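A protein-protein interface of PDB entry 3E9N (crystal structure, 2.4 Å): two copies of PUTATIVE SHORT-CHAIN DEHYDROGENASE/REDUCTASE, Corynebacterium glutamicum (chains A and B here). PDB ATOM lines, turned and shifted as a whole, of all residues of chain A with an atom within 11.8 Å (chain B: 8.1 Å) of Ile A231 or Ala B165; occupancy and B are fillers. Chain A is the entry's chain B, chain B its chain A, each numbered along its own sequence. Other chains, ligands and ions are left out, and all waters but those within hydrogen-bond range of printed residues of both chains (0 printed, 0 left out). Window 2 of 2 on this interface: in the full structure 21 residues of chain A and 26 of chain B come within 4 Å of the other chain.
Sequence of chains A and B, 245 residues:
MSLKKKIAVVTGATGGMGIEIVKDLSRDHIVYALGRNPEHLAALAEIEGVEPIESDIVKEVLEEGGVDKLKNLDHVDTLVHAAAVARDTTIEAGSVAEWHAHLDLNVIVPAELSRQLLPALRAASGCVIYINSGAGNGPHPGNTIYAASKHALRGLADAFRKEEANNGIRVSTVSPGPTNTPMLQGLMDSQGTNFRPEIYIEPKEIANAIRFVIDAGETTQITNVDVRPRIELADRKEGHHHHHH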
ATOM      1  N   PRO A 176       4.405  26.275  -4.433  1.00  0.00           N
ATOM      2  CA  PRO A 176       2.971  26.189  -4.742  1.00  0.00           C
ATOM      3  C   PRO A 176       2.620  25.137  -5.797  1.00  0.00           C
ATOM      4  O   PRO A 176       3.318  24.114  -5.886  1.00  0.00           O
ATOM      5  CB  PRO A 176       2.641  27.607  -5.284  1.00  0.00           C
ATOM      6  CG  PRO A 176       3.959  28.415  -5.160  1.00  0.00           C
ATOM      7  CD  PRO A 176       5.031  27.355  -5.203  1.00  0.00           C
ATOM      8  N   ILE A 201      -4.096  28.188  -7.401  1.00  0.00           N
ATOM      9  CA  ILE A 201      -3.942  28.641  -6.016  1.00  0.00           C
ATOM     10  C   ILE A 201      -4.135  30.174  -5.781  1.00  0.00           C
ATOM     11  O   ILE A 201      -3.429  30.997  -6.345  1.00  0.00           O
ATOM     12  CB  ILE A 201      -2.606  28.121  -5.405  1.00  0.00           C
ATOM     13  CG1 ILE A 201      -2.738  26.609  -5.115  1.00  0.00           C
ATOM     14  CG2 ILE A 201      -2.232  28.905  -4.134  1.00  0.00           C
ATOM     15  CD1 ILE A 201      -1.456  25.855  -4.760  1.00  0.00           C
ATOM     16  N   GLU A 202      -5.096  30.529  -4.942  1.00  0.00           N
ATOM     17  CA  GLU A 202      -5.328  31.927  -4.589  1.00  0.00           C
ATOM     18  C   GLU A 202      -4.046  32.746  -4.348  1.00  0.00           C
ATOM     19  O   GLU A 202      -3.302  32.459  -3.434  1.00  0.00           O
ATOM     20  CB  GLU A 202      -6.255  32.015  -3.354  1.00  0.00           C
ATOM     21  CG  GLU A 202      -7.715  32.148  -3.669  1.00  0.00           C
ATOM     22  CD  GLU A 202      -8.006  33.518  -4.245  1.00  0.00           C
ATOM     23  OE1 GLU A 202      -7.689  34.531  -3.549  1.00  0.00           O
ATOM     24  OE2 GLU A 202      -8.519  33.580  -5.390  1.00  0.00           O
ATOM     25  N   ASP A 226       5.217  24.569   1.777  1.00  0.00           N
ATOM     26  CA  ASP A 226       4.463  23.936   0.712  1.00  0.00           C
ATOM     27  C   ASP A 226       2.986  24.342   0.742  1.00  0.00           C
ATOM     28  O   ASP A 226       2.282  24.147   1.727  1.00  0.00           O
ATOM     29  CB  ASP A 226       4.576  22.407   0.785  1.00  0.00           C
ATOM     30  CG  ASP A 226       6.015  21.905   0.607  1.00  0.00           C
ATOM     31  OD1 ASP A 226       6.393  20.929   1.294  1.00  0.00           O
ATOM     32  OD2 ASP A 226       6.806  22.485  -0.191  1.00  0.00           O
ATOM     33  N   VAL A 227       2.520  24.897  -0.367  1.00  0.00           N
ATOM     34  CA  VAL A 227       1.153  25.326  -0.555  1.00  0.00           C
ATOM     35  C   VAL A 227       0.498  24.431  -1.631  1.00  0.00           C
ATOM     36  O   VAL A 227       1.018  24.288  -2.730  1.00  0.00           O
ATOM     37  CB  VAL A 227       1.202  26.746  -1.016  1.00  0.00           C
ATOM     38  CG1 VAL A 227      -0.174  27.305  -1.258  1.00  0.00           C
ATOM     39  CG2 VAL A 227       1.945  27.580   0.027  1.00  0.00           C
ATOM     40  N   ARG A 228      -0.632  23.801  -1.309  1.00  0.00           N
ATOM     41  CA  ARG A 228      -1.290  22.870  -2.230  1.00  0.00           C
ATOM     42  C   ARG A 228      -2.720  23.270  -2.320  1.00  0.00           C
ATOM     43  O   ARG A 228      -3.228  23.936  -1.419  1.00  0.00           O
ATOM     44  CB  ARG A 228      -1.162  21.407  -1.771  1.00  0.00           C
ATOM     45  CG  ARG A 228       0.089  20.700  -2.339  1.00  0.00           C
ATOM     46  CD  ARG A 228       1.291  20.988  -1.486  1.00  0.00           C
ATOM     47  NE  ARG A 228       2.569  20.451  -1.975  1.00  0.00           N
ATOM     48  CZ  ARG A 228       3.385  21.126  -2.771  1.00  0.00           C
ATOM     49  NH1 ARG A 228       4.543  20.607  -3.137  1.00  0.00           N
ATOM     50  NH2 ARG A 228       3.026  22.330  -3.194  1.00  0.00           N
ATOM     51  N   PRO A 229      -3.376  22.889  -3.425  1.00  0.00           N
ATOM     52  CA  PRO A 229      -4.803  23.124  -3.493  1.00  0.00           C
ATOM     53  C   PRO A 229      -5.459  22.336  -2.356  1.00  0.00           C
ATOM     54  O   PRO A 229      -4.866  21.395  -1.806  1.00  0.00           O
ATOM     55  CB  PRO A 229      -5.225  22.536  -4.857  1.00  0.00           C
ATOM     56  CG  PRO A 229      -4.034  22.022  -5.501  1.00  0.00           C
ATOM     57  CD  PRO A 229      -2.889  22.022  -4.499  1.00  0.00           C
ATOM     58  N   ARG A 230      -6.663  22.729  -1.979  1.00  0.00           N
ATOM     59  CA  ARG A 230      -7.367  21.981  -0.962  1.00  0.00           C
ATOM     60  C   ARG A 230      -7.238  20.468  -1.226  1.00  0.00           C
ATOM     61  O   ARG A 230      -6.723  19.699  -0.397  1.00  0.00           O
ATOM     62  CB  ARG A 230      -8.827  22.421  -0.915  1.00  0.00           C
ATOM     63  CG  ARG A 230      -9.635  21.731   0.155  1.00  0.00           C
ATOM     64  CD  ARG A 230      -8.913  21.684   1.457  1.00  0.00           C
ATOM     65  NE  ARG A 230      -9.797  21.205   2.502  1.00  0.00           N
ATOM     66  CZ  ARG A 230     -10.577  22.008   3.212  1.00  0.00           C
ATOM     67  NH1 ARG A 230     -10.539  23.322   2.964  1.00  0.00           N
ATOM     68  NH2 ARG A 230     -11.360  21.508   4.168  1.00  0.00           N
ATOM     69  N   ILE A 231      -7.714  20.040  -2.387  1.00  0.00           N
ATOM     70  CA  ILE A 231      -7.664  18.606  -2.731  1.00  0.00           C
ATOM     71  C   ILE A 231      -6.823  18.314  -3.981  1.00  0.00           C
ATOM     72  O   ILE A 231      -7.166  18.794  -5.055  1.00  0.00           O
ATOM     73  CB  ILE A 231      -9.076  18.034  -2.982  1.00  0.00           C
ATOM     74  CG1 ILE A 231      -9.970  18.244  -1.758  1.00  0.00           C
ATOM     75  CG2 ILE A 231      -8.965  16.566  -3.353  1.00  0.00           C
ATOM     76  CD1 ILE A 231     -11.426  17.838  -1.980  1.00  0.00           C
ATOM     77  N   SER B 125     -14.603  18.945   9.242  1.00  0.00           N
ATOM     78  CA  SER B 125     -13.528  19.177   8.269  1.00  0.00           C
ATOM     79  C   SER B 125     -12.217  19.738   8.899  1.00  0.00           C
ATOM     80  O   SER B 125     -11.671  20.745   8.436  1.00  0.00           O
ATOM     81  CB  SER B 125     -14.011  20.112   7.148  1.00  0.00           C
ATOM     82  OG  SER B 125     -15.068  19.514   6.447  1.00  0.00           O
ATOM     83  N   ALA B 159       0.402   9.976   3.746  1.00  0.00           N
ATOM     84  CA  ALA B 159      -0.564   8.946   3.261  1.00  0.00           C
ATOM     85  C   ALA B 159      -1.954   9.195   3.869  1.00  0.00           C
ATOM     86  O   ALA B 159      -2.996   8.937   3.244  1.00  0.00           O
ATOM     87  CB  ALA B 159      -0.118   7.573   3.591  1.00  0.00           C
ATOM     88  N   PHE B 160      -1.933   9.697   5.092  1.00  0.00           N
ATOM     89  CA  PHE B 160      -3.130  10.110   5.799  1.00  0.00           C
ATOM     90  C   PHE B 160      -3.814  11.255   5.040  1.00  0.00           C
ATOM     91  O   PHE B 160      -5.039  11.211   4.768  1.00  0.00           O
ATOM     92  CB  PHE B 160      -2.748  10.554   7.221  1.00  0.00           C
ATOM     93  CG  PHE B 160      -3.923  10.841   8.095  1.00  0.00           C
ATOM     94  CD1 PHE B 160      -4.772   9.822   8.481  1.00  0.00           C
ATOM     95  CD2 PHE B 160      -4.192  12.137   8.525  1.00  0.00           C
ATOM     96  CE1 PHE B 160      -5.875  10.098   9.291  1.00  0.00           C
ATOM     97  CE2 PHE B 160      -5.290  12.416   9.346  1.00  0.00           C
ATOM     98  CZ  PHE B 160      -6.130  11.411   9.740  1.00  0.00           C
ATOM     99  N   ARG B 161      -3.025  12.288   4.725  1.00  0.00           N
ATOM    100  CA  ARG B 161      -3.497  13.396   3.886  1.00  0.00           C
ATOM    101  C   ARG B 161      -4.208  12.905   2.648  1.00  0.00           C
ATOM    102  O   ARG B 161      -5.303  13.370   2.371  1.00  0.00           O
ATOM    103  CB  ARG B 161      -2.354  14.374   3.505  1.00  0.00           C
ATOM    104  CG  ARG B 161      -2.792  15.514   2.568  1.00  0.00           C
ATOM    105  CD  ARG B 161      -1.653  16.407   2.179  1.00  0.00           C
ATOM    106  NE  ARG B 161      -0.976  16.939   3.357  1.00  0.00           N
ATOM    107  CZ  ARG B 161       0.230  16.534   3.747  1.00  0.00           C
ATOM    108  NH1 ARG B 161       0.878  15.601   3.025  1.00  0.00           N
ATOM    109  NH2 ARG B 161       0.807  17.084   4.819  1.00  0.00           N
ATOM    110  N   LYS B 162      -3.613  11.952   1.931  1.00  0.00           N
ATOM    111  CA  LYS B 162      -4.225  11.440   0.685  1.00  0.00           C
ATOM    112  C   LYS B 162      -5.470  10.639   0.983  1.00  0.00           C
ATOM    113  O   LYS B 162      -6.439  10.710   0.238  1.00  0.00           O
ATOM    114  CB  LYS B 162      -3.279  10.535  -0.123  1.00  0.00           C
ATOM    115  CG  LYS B 162      -1.932  11.144  -0.567  1.00  0.00           C
ATOM    116  CD  LYS B 162      -0.911  10.006  -0.956  1.00  0.00           C
ATOM    117  CE  LYS B 162      -0.494   9.138   0.298  1.00  0.00           C
ATOM    118  NZ  LYS B 162       0.782   8.292   0.202  1.00  0.00           N
ATOM    119  N   GLU B 163      -5.443   9.847   2.050  1.00  0.00           N
ATOM    120  CA  GLU B 163      -6.637   9.147   2.472  1.00  0.00           C
ATOM    121  C   GLU B 163      -7.804  10.089   2.809  1.00  0.00           C
ATOM    122  O   GLU B 163      -8.952   9.742   2.582  1.00  0.00           O
ATOM    123  CB  GLU B 163      -6.343   8.270   3.682  1.00  0.00           C
ATOM    124  CG  GLU B 163      -5.900   6.860   3.355  1.00  0.00           C
ATOM    125  CD  GLU B 163      -5.716   6.004   4.601  1.00  0.00           C
ATOM    126  OE1 GLU B 163      -5.767   6.546   5.730  1.00  0.00           O
ATOM    127  OE2 GLU B 163      -5.508   4.774   4.466  1.00  0.00           O
ATOM    128  N   GLU B 164      -7.527  11.271   3.373  1.00  0.00           N
ATOM    129  CA  GLU B 164      -8.629  12.059   3.938  1.00  0.00           C
ATOM    130  C   GLU B 164      -8.979  13.364   3.240  1.00  0.00           C
ATOM    131  O   GLU B 164      -9.921  14.034   3.677  1.00  0.00           O
ATOM    132  CB  GLU B 164      -8.392  12.319   5.423  1.00  0.00           C
ATOM    133  CG  GLU B 164      -8.356  11.026   6.242  1.00  0.00           C
ATOM    134  CD  GLU B 164      -9.694  10.309   6.225  1.00  0.00           C
ATOM    135  OE1 GLU B 164     -10.746  10.991   6.119  1.00  0.00           O
ATOM    136  OE2 GLU B 164      -9.701   9.068   6.316  1.00  0.00           O
ATOM    137  N   ALA B 165      -8.239  13.749   2.187  1.00  0.00           N
ATOM    138  CA  ALA B 165      -8.502  15.050   1.509  1.00  0.00           C
ATOM    139  C   ALA B 165      -9.961  15.220   1.083  1.00  0.00           C
ATOM    140  O   ALA B 165     -10.566  16.268   1.341  1.00  0.00           O
ATOM    141  CB  ALA B 165      -7.570  15.259   0.315  1.00  0.00           C
ATOM    142  N   ASN B 166     -10.522  14.188   0.446  1.00  0.00           N
ATOM    143  CA  ASN B 166     -11.945  14.193   0.046  1.00  0.00           C
ATOM    144  C   ASN B 166     -12.958  14.362   1.180  1.00  0.00           C
ATOM    145  O   ASN B 166     -14.113  14.765   0.960  1.00  0.00           O
ATOM    146  CB  ASN B 166     -12.288  12.934  -0.758  1.00  0.00           C
ATOM    147  CG  ASN B 166     -11.768  13.020  -2.170  1.00  0.00           C
ATOM    148  OD1 ASN B 166     -10.788  12.352  -2.516  1.00  0.00           O
ATOM    149  ND2 ASN B 166     -12.365  13.918  -2.979  1.00  0.00           N
ATOM    150  N   ASN B 167     -12.537  14.057   2.401  1.00  0.00           N
ATOM    151  CA  ASN B 167     -13.463  14.216   3.494  1.00  0.00           C
ATOM    152  C   ASN B 167     -13.386  15.558   4.144  1.00  0.00           C
ATOM    153  O   ASN B 167     -14.077  15.783   5.141  1.00  0.00           O
ATOM    154  CB  ASN B 167     -13.268  13.124   4.500  1.00  0.00           C
ATOM    155  CG  ASN B 167     -13.455  11.778   3.882  1.00  0.00           C
ATOM    156  OD1 ASN B 167     -14.411  11.577   3.123  1.00  0.00           O
ATOM    157  ND2 ASN B 167     -12.525  10.862   4.135  1.00  0.00           N
ATOM    158  N   GLY B 168     -12.553  16.455   3.598  1.00  0.00           N
ATOM    159  CA  GLY B 168     -12.534  17.803   4.124  1.00  0.00           C
ATOM    160  C   GLY B 168     -11.445  17.984   5.150  1.00  0.00           C
ATOM    161  O   GLY B 168     -11.286  19.092   5.695  1.00  0.00           O
ATOM    162  N   ILE B 169     -10.690  16.920   5.426  1.00  0.00           N
ATOM    163  CA  ILE B 169      -9.602  17.012   6.393  1.00  0.00           C
ATOM    164  C   ILE B 169      -8.306  17.552   5.790  1.00  0.00           C
ATOM    165  O   ILE B 169      -7.883  17.137   4.698  1.00  0.00           O
ATOM    166  CB  ILE B 169      -9.321  15.655   7.073  1.00  0.00           C
ATOM    167  CG1 ILE B 169     -10.563  15.188   7.869  1.00  0.00           C
ATOM    168  CG2 ILE B 169      -8.040  15.729   7.953  1.00  0.00           C
ATOM    169  CD1 ILE B 169     -10.414  13.836   8.528  1.00  0.00           C
ATOM    170  N   ARG B 170      -7.698  18.510   6.489  1.00  0.00           N
ATOM    171  CA  ARG B 170      -6.420  19.017   6.091  1.00  0.00           C
ATOM    172  C   ARG B 170      -5.349  18.448   7.002  1.00  0.00           C
ATOM    173  O   ARG B 170      -5.549  18.264   8.229  1.00  0.00           O
ATOM    174  CB  ARG B 170      -6.417  20.563   6.060  1.00  0.00           C
ATOM    175  CG  ARG B 170      -7.532  21.123   5.112  1.00  0.00           C
ATOM    176  CD  ARG B 170      -7.368  22.612   4.845  1.00  0.00           C
ATOM    177  NE  ARG B 170      -7.686  23.465   5.993  1.00  0.00           N
ATOM    178  CZ  ARG B 170      -7.735  24.803   5.965  1.00  0.00           C
ATOM    179  NH1 ARG B 170      -7.487  25.500   4.840  1.00  0.00           N
ATOM    180  NH2 ARG B 170      -8.032  25.454   7.079  1.00  0.00           N
ATOM    181  N   VAL B 171      -4.208  18.127   6.392  1.00  0.00           N
ATOM    182  CA  VAL B 171      -3.146  17.486   7.103  1.00  0.00           C
ATOM    183  C   VAL B 171      -1.876  18.281   6.854  1.00  0.00           C
ATOM    184  O   VAL B 171      -1.572  18.635   5.724  1.00  0.00           O
ATOM    185  CB  VAL B 171      -2.979  16.051   6.677  1.00  0.00           C
ATOM    186  CG1 VAL B 171      -1.890  15.394   7.538  1.00  0.00           C
ATOM    187  CG2 VAL B 171      -4.284  15.283   6.875  1.00  0.00           C
ATOM    188  N   GLU B 218      -9.779  28.330   2.181  1.00  0.00           N
ATOM    189  CA  GLU B 218     -10.430  27.043   1.969  1.00  0.00           C
ATOM    190  C   GLU B 218      -9.972  26.330   0.722  1.00  0.00           C
ATOM    191  O   GLU B 218     -10.063  25.113   0.663  1.00  0.00           O
ATOM    192  CB  GLU B 218     -11.940  27.226   1.873  1.00  0.00           C
ATOM    193  CG  GLU B 218     -12.609  27.677   3.163  1.00  0.00           C
ATOM    194  CD  GLU B 218     -13.010  26.473   3.999  1.00  0.00           C
ATOM    195  OE1 GLU B 218     -12.682  26.412   5.210  1.00  0.00           O
ATOM    196  OE2 GLU B 218     -13.634  25.563   3.405  1.00  0.00           O
ATOM    197  N   THR B 219      -9.478  27.071  -0.269  1.00  0.00           N
ATOM    198  CA  THR B 219      -8.972  26.439  -1.472  1.00  0.00           C
ATOM    199  C   THR B 219      -7.549  25.953  -1.286  1.00  0.00           C
ATOM    200  O   THR B 219      -6.947  25.452  -2.218  1.00  0.00           O
ATOM    201  CB  THR B 219      -8.932  27.391  -2.687  1.00  0.00           C
ATOM    202  OG1 THR B 219      -7.831  28.287  -2.531  1.00  0.00           O
ATOM    203  CG2 THR B 219     -10.195  28.153  -2.831  1.00  0.00           C
ATOM    204  N   THR B 220      -7.033  26.048  -0.072  1.00  0.00           N
ATOM    205  CA  THR B 220      -5.609  25.772   0.184  1.00  0.00           C
ATOM    206  C   THR B 220      -5.364  24.774   1.312  1.00  0.00           C
ATOM    207  O   THR B 220      -6.229  24.560   2.156  1.00  0.00           O
ATOM    208  CB  THR B 220      -4.891  27.064   0.503  1.00  0.00           C
ATOM    209  OG1 THR B 220      -5.464  28.103  -0.303  1.00  0.00           O
ATOM    210  CG2 THR B 220      -3.444  26.963   0.163  1.00  0.00           C
ATOM    211  N   GLN B 221      -4.213  24.107   1.236  1.00  0.00           N
ATOM    212  CA  GLN B 221      -3.615  23.282   2.286  1.00  0.00           C
ATOM    213  C   GLN B 221      -2.160  23.753   2.399  1.00  0.00           C
ATOM    214  O   GLN B 221      -1.428  23.737   1.413  1.00  0.00           O
ATOM    215  CB  GLN B 221      -3.550  21.793   1.883  1.00  0.00           C
ATOM    216  CG  GLN B 221      -4.828  21.030   1.965  1.00  0.00           C
ATOM    217  CD  GLN B 221      -4.695  19.622   2.571  1.00  0.00           C
ATOM    218  OE1 GLN B 221      -5.387  18.697   2.142  1.00  0.00           O
ATOM    219  NE2 GLN B 221      -3.862  19.469   3.587  1.00  0.00           N
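No position is printed for both chains. Of the 14 pairs that touch across the chains among the printed residues, none has its exchanged pair printed and touching as well.
The side-chain hydroxyl of Thr B220 sits close to the side-chain hydroxyl of Thr B219 (3.3 Å). The guanidinium group of Arg B170 lies within hydrogen-bond range of the backbone carbonyl oxygen of Thr B220. The backbone carbonyl oxygen (O) of Pro A176 sits at hydrogen-bond distance from the guanidinium group (NH2) of Arg A228 (3.2 Å). The backbone NH of Val B171 lies close to the side-chain amide nitrogen of Gln B221.
O of Gln B221 sits at hydrogen-bond distance from N of Arg A228, 2.8 Å away. O of Thr B219 is in hydrogen-bond range of N of Arg A230, 2.7 Å away. The backbone carbonyl oxygen (O) of Gly B168 is in hydrogen-bond range of the guanidinium group (NH2) of Arg A230, at 2.9 Å. The side-chain amide oxygen of Gln B221 lies close to the backbone carbonyl oxygen of Arg A230, 3.0 Å away. The guanidinium group (NH1) of Arg A230 is in salt-bridge range of the side-chain carboxylate (OE2) of Glu B218 (3.8 Å).
Of chain B, only Ala B165 comes within 4 Å of Ile A231. Of chain A, only Ile A231 comes within 4 Å of Ala B165. No residue of chain A comes within 4 Å of Glu B164. No residue of chain A comes within 4 Å of Asn B167. No residue of chain A comes within 4 Å of Ile B169. Of the printed residues of chain A, Thr B220 touches Val A227 (3.6 Å), Arg A228 (3.4 Å) and Arg A230 (3.8 Å). Of the printed residues of chain A, Thr B219 touches Pro A229 and Arg A230. Ile A201 touches none of the printed residues of chain B. Ala B159 touches none of the printed residues of chain A. The nearest residue of chain A that does not touch Ala B165 is Arg A230 (4.6 Å).
Of the 9 printed residues of chain A, 6 touch a printed residue of chain B. Hydrophobic or aromatic side chains of chain A within 4 Å of the printed part of chain B: Val A227 and Ile A231. Along chain B the printed residues that touch a printed residue of chain A span positions 165 to 221. Among the printed residues, 14 pairs touch across the chains.
Among the printed residues, pairs that only touch across the chains: Asp A226 with Gln B221, Val A227 with Thr B220, Val A227 with Gln B221, Arg A228 with Thr B220, Pro A229 with Thr B219, Pro A229 with Gln B221, Arg A230 with Arg B170, Arg A230 with Thr B220 and Ile A231 with Ala B165.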
